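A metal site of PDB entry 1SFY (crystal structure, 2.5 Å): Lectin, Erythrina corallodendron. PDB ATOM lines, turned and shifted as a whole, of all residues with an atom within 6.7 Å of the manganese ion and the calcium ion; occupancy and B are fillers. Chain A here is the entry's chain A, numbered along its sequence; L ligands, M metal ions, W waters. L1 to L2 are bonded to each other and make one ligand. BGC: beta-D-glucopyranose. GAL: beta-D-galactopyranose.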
ATOM      1  N   ASP A  89     -23.331  -0.626  18.955  1.00  0.00           N
ATOM      2  CA  ASP A  89     -23.702  -1.667  17.990  1.00  0.00           C
ATOM      3  C   ASP A  89     -22.709  -2.833  17.929  1.00  0.00           C
ATOM      4  O   ASP A  89     -23.092  -3.956  17.572  1.00  0.00           O
ATOM      5  CB  ASP A  89     -23.833  -1.039  16.599  1.00  0.00           C
ATOM      6  CG  ASP A  89     -25.212  -0.502  16.321  1.00  0.00           C
ATOM      7  OD1 ASP A  89     -26.126  -1.321  16.048  1.00  0.00           O
ATOM      8  OD2 ASP A  89     -25.400   0.734  16.406  1.00  0.00           O
ATOM      9  N   TYR A 106     -23.819   2.454  12.926  1.00  0.00           N
ATOM     10  CA  TYR A 106     -24.857   1.616  13.502  1.00  0.00           C
ATOM     11  C   TYR A 106     -24.659   0.136  13.177  1.00  0.00           C
ATOM     12  O   TYR A 106     -23.548  -0.380  13.236  1.00  0.00           O
ATOM     13  CB  TYR A 106     -26.234   2.065  13.006  1.00  0.00           C
ATOM     14  CG  TYR A 106     -26.454   3.558  13.070  1.00  0.00           C
ATOM     15  CD1 TYR A 106     -26.143   4.281  14.217  1.00  0.00           C
ATOM     16  CD2 TYR A 106     -27.009   4.244  11.991  1.00  0.00           C
ATOM     17  CE1 TYR A 106     -26.367   5.651  14.295  1.00  0.00           C
ATOM     18  CE2 TYR A 106     -27.237   5.617  12.046  1.00  0.00           C
ATOM     19  CZ  TYR A 106     -26.915   6.311  13.201  1.00  0.00           C
ATOM     20  OH  TYR A 106     -27.155   7.662  13.256  1.00  0.00           O
ATOM     21  N   GLY A 107     -25.745  -0.535  12.824  1.00  0.00           N
ATOM     22  CA  GLY A 107     -25.675  -1.953  12.505  1.00  0.00           C
ATOM     23  C   GLY A 107     -24.693  -2.322  11.399  1.00  0.00           C
ATOM     24  O   GLY A 107     -24.327  -3.475  11.266  1.00  0.00           O
ATOM     25  N   TYR A 108     -24.274  -1.339  10.615  1.00  0.00           N
ATOM     26  CA  TYR A 108     -23.334  -1.608   9.526  1.00  0.00           C
ATOM     27  C   TYR A 108     -21.895  -1.601  10.018  1.00  0.00           C
ATOM     28  O   TYR A 108     -20.951  -1.833   9.241  1.00  0.00           O
ATOM     29  CB  TYR A 108     -23.547  -0.602   8.396  1.00  0.00           C
ATOM     30  CG  TYR A 108     -24.947  -0.711   7.823  1.00  0.00           C
ATOM     31  CD1 TYR A 108     -25.362  -1.866   7.170  1.00  0.00           C
ATOM     32  CD2 TYR A 108     -25.878   0.313   8.020  1.00  0.00           C
ATOM     33  CE1 TYR A 108     -26.674  -2.019   6.735  1.00  0.00           C
ATOM     34  CE2 TYR A 108     -27.191   0.169   7.581  1.00  0.00           C
ATOM     35  CZ  TYR A 108     -27.584  -0.993   6.936  1.00  0.00           C
ATOM     36  OH  TYR A 108     -28.892  -1.139   6.520  1.00  0.00           O
ATOM     37  N   LEU A 109     -21.740  -1.339  11.312  1.00  0.00           N
ATOM     38  CA  LEU A 109     -20.439  -1.337  11.978  1.00  0.00           C
ATOM     39  C   LEU A 109     -19.346  -0.503  11.326  1.00  0.00           C
ATOM     40  O   LEU A 109     -18.167  -0.709  11.594  1.00  0.00           O
ATOM     41  CB  LEU A 109     -19.965  -2.776  12.141  1.00  0.00           C
ATOM     42  CG  LEU A 109     -20.992  -3.678  12.836  1.00  0.00           C
ATOM     43  CD1 LEU A 109     -20.416  -5.069  13.035  1.00  0.00           C
ATOM     44  CD2 LEU A 109     -21.382  -3.072  14.181  1.00  0.00           C
ATOM     45  N   GLU A 127     -17.190 -10.023  13.159  1.00  0.00           N
ATOM     46  CA  GLU A 127     -17.914  -9.129  14.051  1.00  0.00           C
ATOM     47  C   GLU A 127     -18.260  -9.654  15.435  1.00  0.00           C
ATOM     48  O   GLU A 127     -18.417 -10.854  15.653  1.00  0.00           O
ATOM     49  CB  GLU A 127     -19.212  -8.662  13.389  1.00  0.00           C
ATOM     50  CG  GLU A 127     -20.134  -9.821  13.056  1.00  0.00           C
ATOM     51  CD  GLU A 127     -21.535  -9.377  12.697  1.00  0.00           C
ATOM     52  OE1 GLU A 127     -21.690  -8.536  11.787  1.00  0.00           O
ATOM     53  OE2 GLU A 127     -22.475  -9.889  13.318  1.00  0.00           O
ATOM     54  N   ASP A 129     -21.096  -8.493  17.428  1.00  0.00           N
ATOM     55  CA  ASP A 129     -22.362  -7.771  17.362  1.00  0.00           C
ATOM     56  C   ASP A 129     -23.149  -7.734  18.653  1.00  0.00           C
ATOM     57  O   ASP A 129     -23.462  -8.782  19.220  1.00  0.00           O
ATOM     58  CB  ASP A 129     -23.216  -8.427  16.290  1.00  0.00           C
ATOM     59  CG  ASP A 129     -24.244  -7.500  15.739  1.00  0.00           C
ATOM     60  OD1 ASP A 129     -24.713  -6.621  16.482  1.00  0.00           O
ATOM     61  OD2 ASP A 129     -24.597  -7.665  14.552  1.00  0.00           O
ATOM     62  N   THR A 130     -23.487  -6.539  19.112  1.00  0.00           N
ATOM     63  CA  THR A 130     -24.225  -6.398  20.365  1.00  0.00           C
ATOM     64  C   THR A 130     -25.692  -5.980  20.236  1.00  0.00           C
ATOM     65  O   THR A 130     -26.415  -5.919  21.233  1.00  0.00           O
ATOM     66  CB  THR A 130     -23.514  -5.401  21.303  1.00  0.00           C
ATOM     67  OG1 THR A 130     -23.373  -4.136  20.642  1.00  0.00           O
ATOM     68  CG2 THR A 130     -22.153  -5.922  21.688  1.00  0.00           C
ATOM     69  N   PHE A 131     -26.132  -5.701  19.017  1.00  0.00           N
ATOM     70  CA  PHE A 131     -27.520  -5.317  18.785  1.00  0.00           C
ATOM     71  C   PHE A 131     -28.129  -6.199  17.718  1.00  0.00           C
ATOM     72  O   PHE A 131     -27.502  -6.481  16.703  1.00  0.00           O
ATOM     73  CB  PHE A 131     -27.617  -3.858  18.357  1.00  0.00           C
ATOM     74  CG  PHE A 131     -29.029  -3.389  18.187  1.00  0.00           C
ATOM     75  CD1 PHE A 131     -29.774  -2.982  19.292  1.00  0.00           C
ATOM     76  CD2 PHE A 131     -29.631  -3.380  16.938  1.00  0.00           C
ATOM     77  CE1 PHE A 131     -31.112  -2.576  19.150  1.00  0.00           C
ATOM     78  CE2 PHE A 131     -30.963  -2.990  16.779  1.00  0.00           C
ATOM     79  CZ  PHE A 131     -31.696  -2.580  17.891  1.00  0.00           C
ATOM     80  N   SER A 132     -29.375  -6.633  17.923  1.00  0.00           N
ATOM     81  CA  SER A 132     -30.028  -7.488  16.933  1.00  0.00           C
ATOM     82  C   SER A 132     -30.826  -6.699  15.891  1.00  0.00           C
ATOM     83  O   SER A 132     -31.894  -6.182  16.192  1.00  0.00           O
ATOM     84  CB  SER A 132     -30.937  -8.494  17.627  1.00  0.00           C
ATOM     85  OG  SER A 132     -31.409  -9.460  16.701  1.00  0.00           O
ATOM     86  N   ASN A 133     -30.293  -6.618  14.680  1.00  0.00           N
ATOM     87  CA  ASN A 133     -30.943  -5.909  13.580  1.00  0.00           C
ATOM     88  C   ASN A 133     -31.861  -6.870  12.817  1.00  0.00           C
ATOM     89  O   ASN A 133     -31.882  -8.065  13.100  1.00  0.00           O
ATOM     90  CB  ASN A 133     -29.901  -5.317  12.636  1.00  0.00           C
ATOM     91  CG  ASN A 133     -29.260  -4.052  13.167  1.00  0.00           C
ATOM     92  OD1 ASN A 133     -28.610  -4.063  14.200  1.00  0.00           O
ATOM     93  ND2 ASN A 133     -29.469  -2.943  12.478  1.00  0.00           N
ATOM     94  N   TRP A 135     -31.557  -8.168  10.068  1.00  0.00           N
ATOM     95  CA  TRP A 135     -30.760  -9.199   9.415  1.00  0.00           C
ATOM     96  C   TRP A 135     -29.993 -10.100  10.384  1.00  0.00           C
ATOM     97  O   TRP A 135     -29.320 -11.033   9.952  1.00  0.00           O
ATOM     98  CB  TRP A 135     -29.795  -8.548   8.434  1.00  0.00           C
ATOM     99  CG  TRP A 135     -28.836  -7.600   9.096  1.00  0.00           C
ATOM    100  CD1 TRP A 135     -27.763  -7.915   9.872  1.00  0.00           C
ATOM    101  CD2 TRP A 135     -28.909  -6.169   9.096  1.00  0.00           C
ATOM    102  NE1 TRP A 135     -27.160  -6.776  10.349  1.00  0.00           N
ATOM    103  CE2 TRP A 135     -27.844  -5.691   9.892  1.00  0.00           C
ATOM    104  CE3 TRP A 135     -29.773  -5.235   8.495  1.00  0.00           C
ATOM    105  CZ2 TRP A 135     -27.622  -4.328  10.101  1.00  0.00           C
ATOM    106  CZ3 TRP A 135     -29.550  -3.881   8.707  1.00  0.00           C
ATOM    107  CH2 TRP A 135     -28.487  -3.444   9.508  1.00  0.00           C
ATOM    108  N   ASP A 136     -30.084  -9.843  11.680  1.00  0.00           N
ATOM    109  CA  ASP A 136     -29.359 -10.653  12.669  1.00  0.00           C
ATOM    110  C   ASP A 136     -30.191 -11.740  13.310  1.00  0.00           C
ATOM    111  O   ASP A 136     -31.410 -11.703  13.285  1.00  0.00           O
ATOM    112  CB  ASP A 136     -28.835  -9.794  13.828  1.00  0.00           C
ATOM    113  CG  ASP A 136     -27.638  -8.929  13.674  1.00  0.00           C
ATOM    114  OD1 ASP A 136     -26.591  -9.427  13.219  1.00  0.00           O
ATOM    115  OD2 ASP A 136     -27.733  -7.744  14.028  1.00  0.00           O
ATOM    116  N   PRO A 137     -29.516 -12.736  13.899  1.00  0.00           N
ATOM    117  CA  PRO A 137     -30.252 -13.804  14.556  1.00  0.00           C
ATOM    118  C   PRO A 137     -30.752 -13.134  15.848  1.00  0.00           C
ATOM    119  O   PRO A 137     -30.289 -12.052  16.203  1.00  0.00           O
ATOM    120  CB  PRO A 137     -29.177 -14.854  14.815  1.00  0.00           C
ATOM    121  CG  PRO A 137     -27.928 -14.060  14.936  1.00  0.00           C
ATOM    122  CD  PRO A 137     -28.080 -13.073  13.810  1.00  0.00           C
ATOM    123  N   VAL A 140     -27.937 -11.954  20.987  1.00  0.00           N
ATOM    124  CA  VAL A 140     -26.871 -10.964  21.013  1.00  0.00           C
ATOM    125  C   VAL A 140     -26.335 -10.966  22.437  1.00  0.00           C
ATOM    126  O   VAL A 140     -27.082 -11.178  23.385  1.00  0.00           O
ATOM    127  CB  VAL A 140     -27.356  -9.534  20.649  1.00  0.00           C
ATOM    128  CG1 VAL A 140     -27.694  -9.450  19.174  1.00  0.00           C
ATOM    129  CG2 VAL A 140     -28.560  -9.148  21.516  1.00  0.00           C
ATOM    130  N   HIS A 142     -23.229 -11.672  19.558  1.00  0.00           N
ATOM    131  CA  HIS A 142     -22.839 -12.855  18.800  1.00  0.00           C
ATOM    132  C   HIS A 142     -21.617 -12.553  17.954  1.00  0.00           C
ATOM    133  O   HIS A 142     -21.373 -11.409  17.574  1.00  0.00           O
ATOM    134  CB  HIS A 142     -23.985 -13.347  17.908  1.00  0.00           C
ATOM    135  CG  HIS A 142     -24.433 -12.354  16.878  1.00  0.00           C
ATOM    136  ND1 HIS A 142     -25.584 -11.600  17.015  1.00  0.00           N
ATOM    137  CD2 HIS A 142     -23.907 -12.016  15.673  1.00  0.00           C
ATOM    138  CE1 HIS A 142     -25.744 -10.836  15.949  1.00  0.00           C
ATOM    139  NE2 HIS A 142     -24.741 -11.076  15.118  1.00  0.00           N
ATOM    140  N   ILE A 143     -20.832 -13.592  17.697  1.00  0.00           N
ATOM    141  CA  ILE A 143     -19.652 -13.476  16.840  1.00  0.00           C
ATOM    142  C   ILE A 143     -20.178 -13.822  15.452  1.00  0.00           C
ATOM    143  O   ILE A 143     -21.015 -14.726  15.323  1.00  0.00           O
ATOM    144  CB  ILE A 143     -18.557 -14.503  17.194  1.00  0.00           C
ATOM    145  CG1 ILE A 143     -18.189 -14.385  18.667  1.00  0.00           C
ATOM    146  CG2 ILE A 143     -17.345 -14.284  16.325  1.00  0.00           C
ATOM    147  CD1 ILE A 143     -17.260 -15.484  19.128  1.00  0.00           C
ATOM    148  N   GLY A 144     -19.718 -13.121  14.435  1.00  0.00           N
ATOM    149  CA  GLY A 144     -20.198 -13.414  13.105  1.00  0.00           C
ATOM    150  C   GLY A 144     -19.115 -13.248  12.067  1.00  0.00           C
ATOM    151  O   GLY A 144     -18.252 -12.371  12.178  1.00  0.00           O
ATOM    152  N   ASP A 146     -18.461 -12.213   8.421  1.00  0.00           N
ATOM    153  CA  ASP A 146     -19.070 -11.429   7.351  1.00  0.00           C
ATOM    154  C   ASP A 146     -18.282 -11.434   6.059  1.00  0.00           C
ATOM    155  O   ASP A 146     -17.135 -11.008   6.020  1.00  0.00           O
ATOM    156  CB  ASP A 146     -19.283  -9.986   7.812  1.00  0.00           C
ATOM    157  CG  ASP A 146     -20.089  -9.889   9.096  1.00  0.00           C
ATOM    158  OD1 ASP A 146     -20.744 -10.882   9.480  1.00  0.00           O
ATOM    159  OD2 ASP A 146     -20.081  -8.815   9.728  1.00  0.00           O
ATOM    160  N   ILE A 150     -23.305  -7.561   5.703  1.00  0.00           N
ATOM    161  CA  ILE A 150     -23.465  -7.437   7.138  1.00  0.00           C
ATOM    162  C   ILE A 150     -24.247  -8.643   7.649  1.00  0.00           C
ATOM    163  O   ILE A 150     -24.291  -8.907   8.850  1.00  0.00           O
ATOM    164  CB  ILE A 150     -24.224  -6.143   7.514  1.00  0.00           C
ATOM    165  CG1 ILE A 150     -24.200  -5.933   9.029  1.00  0.00           C
ATOM    166  CG2 ILE A 150     -25.659  -6.208   7.009  1.00  0.00           C
ATOM    167  CD1 ILE A 150     -22.813  -5.744   9.619  1.00  0.00           C
ATOM    168  N   ARG A 151     -24.878  -9.374   6.738  1.00  0.00           N
ATOM    169  CA  ARG A 151     -25.616 -10.573   7.117  1.00  0.00           C
ATOM    170  C   ARG A 151     -24.637 -11.733   7.133  1.00  0.00           C
ATOM    171  O   ARG A 151     -24.316 -12.306   6.096  1.00  0.00           O
ATOM    172  CB  ARG A 151     -26.801 -10.968   6.263  1.00  0.00           C
ATOM    173  CG  ARG A 151     -27.690 -12.076   6.729  1.00  0.00           C
ATOM    174  CD  ARG A 151     -29.153 -12.010   6.205  1.00  0.00           C
ATOM    175  NE  ARG A 151     -29.792 -11.160   5.173  1.00  0.00           N
ATOM    176  CZ  ARG A 151     -29.565  -9.880   4.878  1.00  0.00           C
ATOM    177  NH1 ARG A 151     -28.560  -9.494   4.103  1.00  0.00           N
ATOM    178  NH2 ARG A 151     -30.373  -8.979   5.406  1.00  0.00           N
ATOM    179  N   SER A 152     -24.156 -12.075   8.322  1.00  0.00           N
ATOM    180  CA  SER A 152     -23.178 -13.141   8.511  1.00  0.00           C
ATOM    181  C   SER A 152     -23.541 -14.466   7.853  1.00  0.00           C
ATOM    182  O   SER A 152     -24.715 -14.822   7.796  1.00  0.00           O
ATOM    183  CB  SER A 152     -22.956 -13.391  10.007  1.00  0.00           C
ATOM    184  OG  SER A 152     -22.667 -12.189  10.682  1.00  0.00           O
ATOM    185  N   THR A 155     -22.856 -17.611  12.461  1.00  0.00           N
ATOM    186  CA  THR A 155     -23.048 -16.862  13.689  1.00  0.00           C
ATOM    187  C   THR A 155     -22.837 -17.722  14.929  1.00  0.00           C
ATOM    188  O   THR A 155     -23.053 -18.932  14.913  1.00  0.00           O
ATOM    189  CB  THR A 155     -24.479 -16.258  13.691  1.00  0.00           C
ATOM    190  OG1 THR A 155     -24.412 -14.881  13.289  1.00  0.00           O
ATOM    191  CG2 THR A 155     -25.140 -16.399  15.040  1.00  0.00           C
HETATM  192  C2  BGC L   1     -34.797   4.465  15.878  1.00  0.00           C
HETATM  193  C3  BGC L   1     -33.345   4.100  15.622  1.00  0.00           C
HETATM  194  C4  BGC L   1     -33.345   2.789  14.737  1.00  0.00           C
HETATM  195  C5  BGC L   1     -34.121   2.993  13.391  1.00  0.00           C
HETATM  196  C6  BGC L   1     -34.377   1.733  12.491  1.00  0.00           C
HETATM  197  C1  BGC L   1     -35.501   4.711  14.523  1.00  0.00           C
HETATM  198  O1  BGC L   1     -36.860   5.047  14.693  1.00  0.00           O
HETATM  199  O2  BGC L   1     -34.829   5.634  16.691  1.00  0.00           O
HETATM  200  O3  BGC L   1     -32.680   3.892  16.874  1.00  0.00           O
HETATM  201  O4  BGC L   1     -31.982   2.394  14.403  1.00  0.00           O
HETATM  202  O5  BGC L   1     -35.434   3.533  13.684  1.00  0.00           O
HETATM  203  O6  BGC L   1     -35.172   0.722  13.194  1.00  0.00           O
HETATM  204  C1  GAL L   2     -31.359   1.321  15.107  1.00  0.00           C
HETATM  205  C2  GAL L   2     -30.098   0.885  14.332  1.00  0.00           C
HETATM  206  C3  GAL L   2     -29.406  -0.281  15.098  1.00  0.00           C
HETATM  207  C4  GAL L   2     -29.055   0.248  16.535  1.00  0.00           C
HETATM  208  C5  GAL L   2     -30.345   0.710  17.263  1.00  0.00           C
HETATM  209  C6  GAL L   2     -30.071   1.279  18.669  1.00  0.00           C
HETATM  210  O2  GAL L   2     -30.408   0.443  13.019  1.00  0.00           O
HETATM  211  O3  GAL L   2     -28.222  -0.706  14.391  1.00  0.00           O
HETATM  212  O4  GAL L   2     -28.109   1.344  16.451  1.00  0.00           O
HETATM  213  O5  GAL L   2     -31.002   1.734  16.454  1.00  0.00           O
HETATM  214  O6  GAL L   2     -31.292   1.658  19.249  1.00  0.00           O
HETATM  215 MN    MN M   1     -24.708  -9.639  13.333  1.00  0.00          MN
HETATM  216 CA    CA M   2     -26.352  -5.663  14.535  1.00  0.00          CA
HETATM  217  O   HOH W   1     -25.034  -5.243  12.582  1.00  0.00           O
HETATM  218  O   HOH W   2     -24.433  -8.127  11.565  1.00  0.00           O
HETATM  219  O   HOH W   3     -25.036  -3.693  15.900  1.00  0.00           O
HETATM  220  O   HOH W   4     -24.812 -11.429  12.155  1.00  0.00           O
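The manganese ion is bound by OD1 of Asp 136 (1.9 Å), water W4 (2.1 Å), OE2 of Glu 127 (2.2 Å), NE2 of His 142 (2.3 Å), OD2 of Asp 129 (2.3 Å) and water W2 (2.3 Å).
The manganese ion has six donor atoms within binding distance.
Water W2 lies within hydrogen-bond range of OE1 of Glu 127 (2.8 Å), O of Ile 150 (2.8 Å) and NE1 of Trp 135 (3.3 Å).
Of the 23 residues printed, 4 come within 4 Å of the manganese ion.
The nearest printed residue that does not touch the manganese ion is Ser 152 (4.2 Å).
The backbone NH of Glu 127 is in hydrogen-bond range of the backbone carbonyl oxygen of Gly 144 (2.8 Å).
The side-chain carboxylate of Glu 127 sits close to the side-chain carboxylate of Asp 146.
Water W1 is bound to the calcium ion, at 2.4 Å.
The calcium ion is bound by OD2 of Asp 136 (2.5 Å).
O of Phe 131 binds the calcium ion (2.6 Å).
OD2 of Asp 129 binds the calcium ion, at 2.7 Å.
The side-chain carboxylate (OD1) of Asp 129 is bound to the calcium ion (2.7 Å).
Water W3 is bound to the calcium ion (2.7 Å).
The side-chain amide oxygen (OD1) of Asn 133 is bound to the calcium ion, 2.8 Å away.
The calcium ion has seven donor atoms within binding distance.
O3 of GAL L2 sits at hydrogen-bond distance from N of Gly 107.
The side-chain amide nitrogen of Asn 133 lies within hydrogen-bond range of an oxygen (O3) of GAL L2.
O3 of GAL L2 is in hydrogen-bond range of OD1 of Asp 89, 2.7 Å away.
Four residues have an atom within 4 Å of the calcium ion: Asp 129, Phe 131, Asn 133 and Asp 136.
Along chain A the residues within 4 Å of the calcium ion span positions 129 to 136.
The nearest printed residue that does not touch the calcium ion is Gly 107 (4.3 Å).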
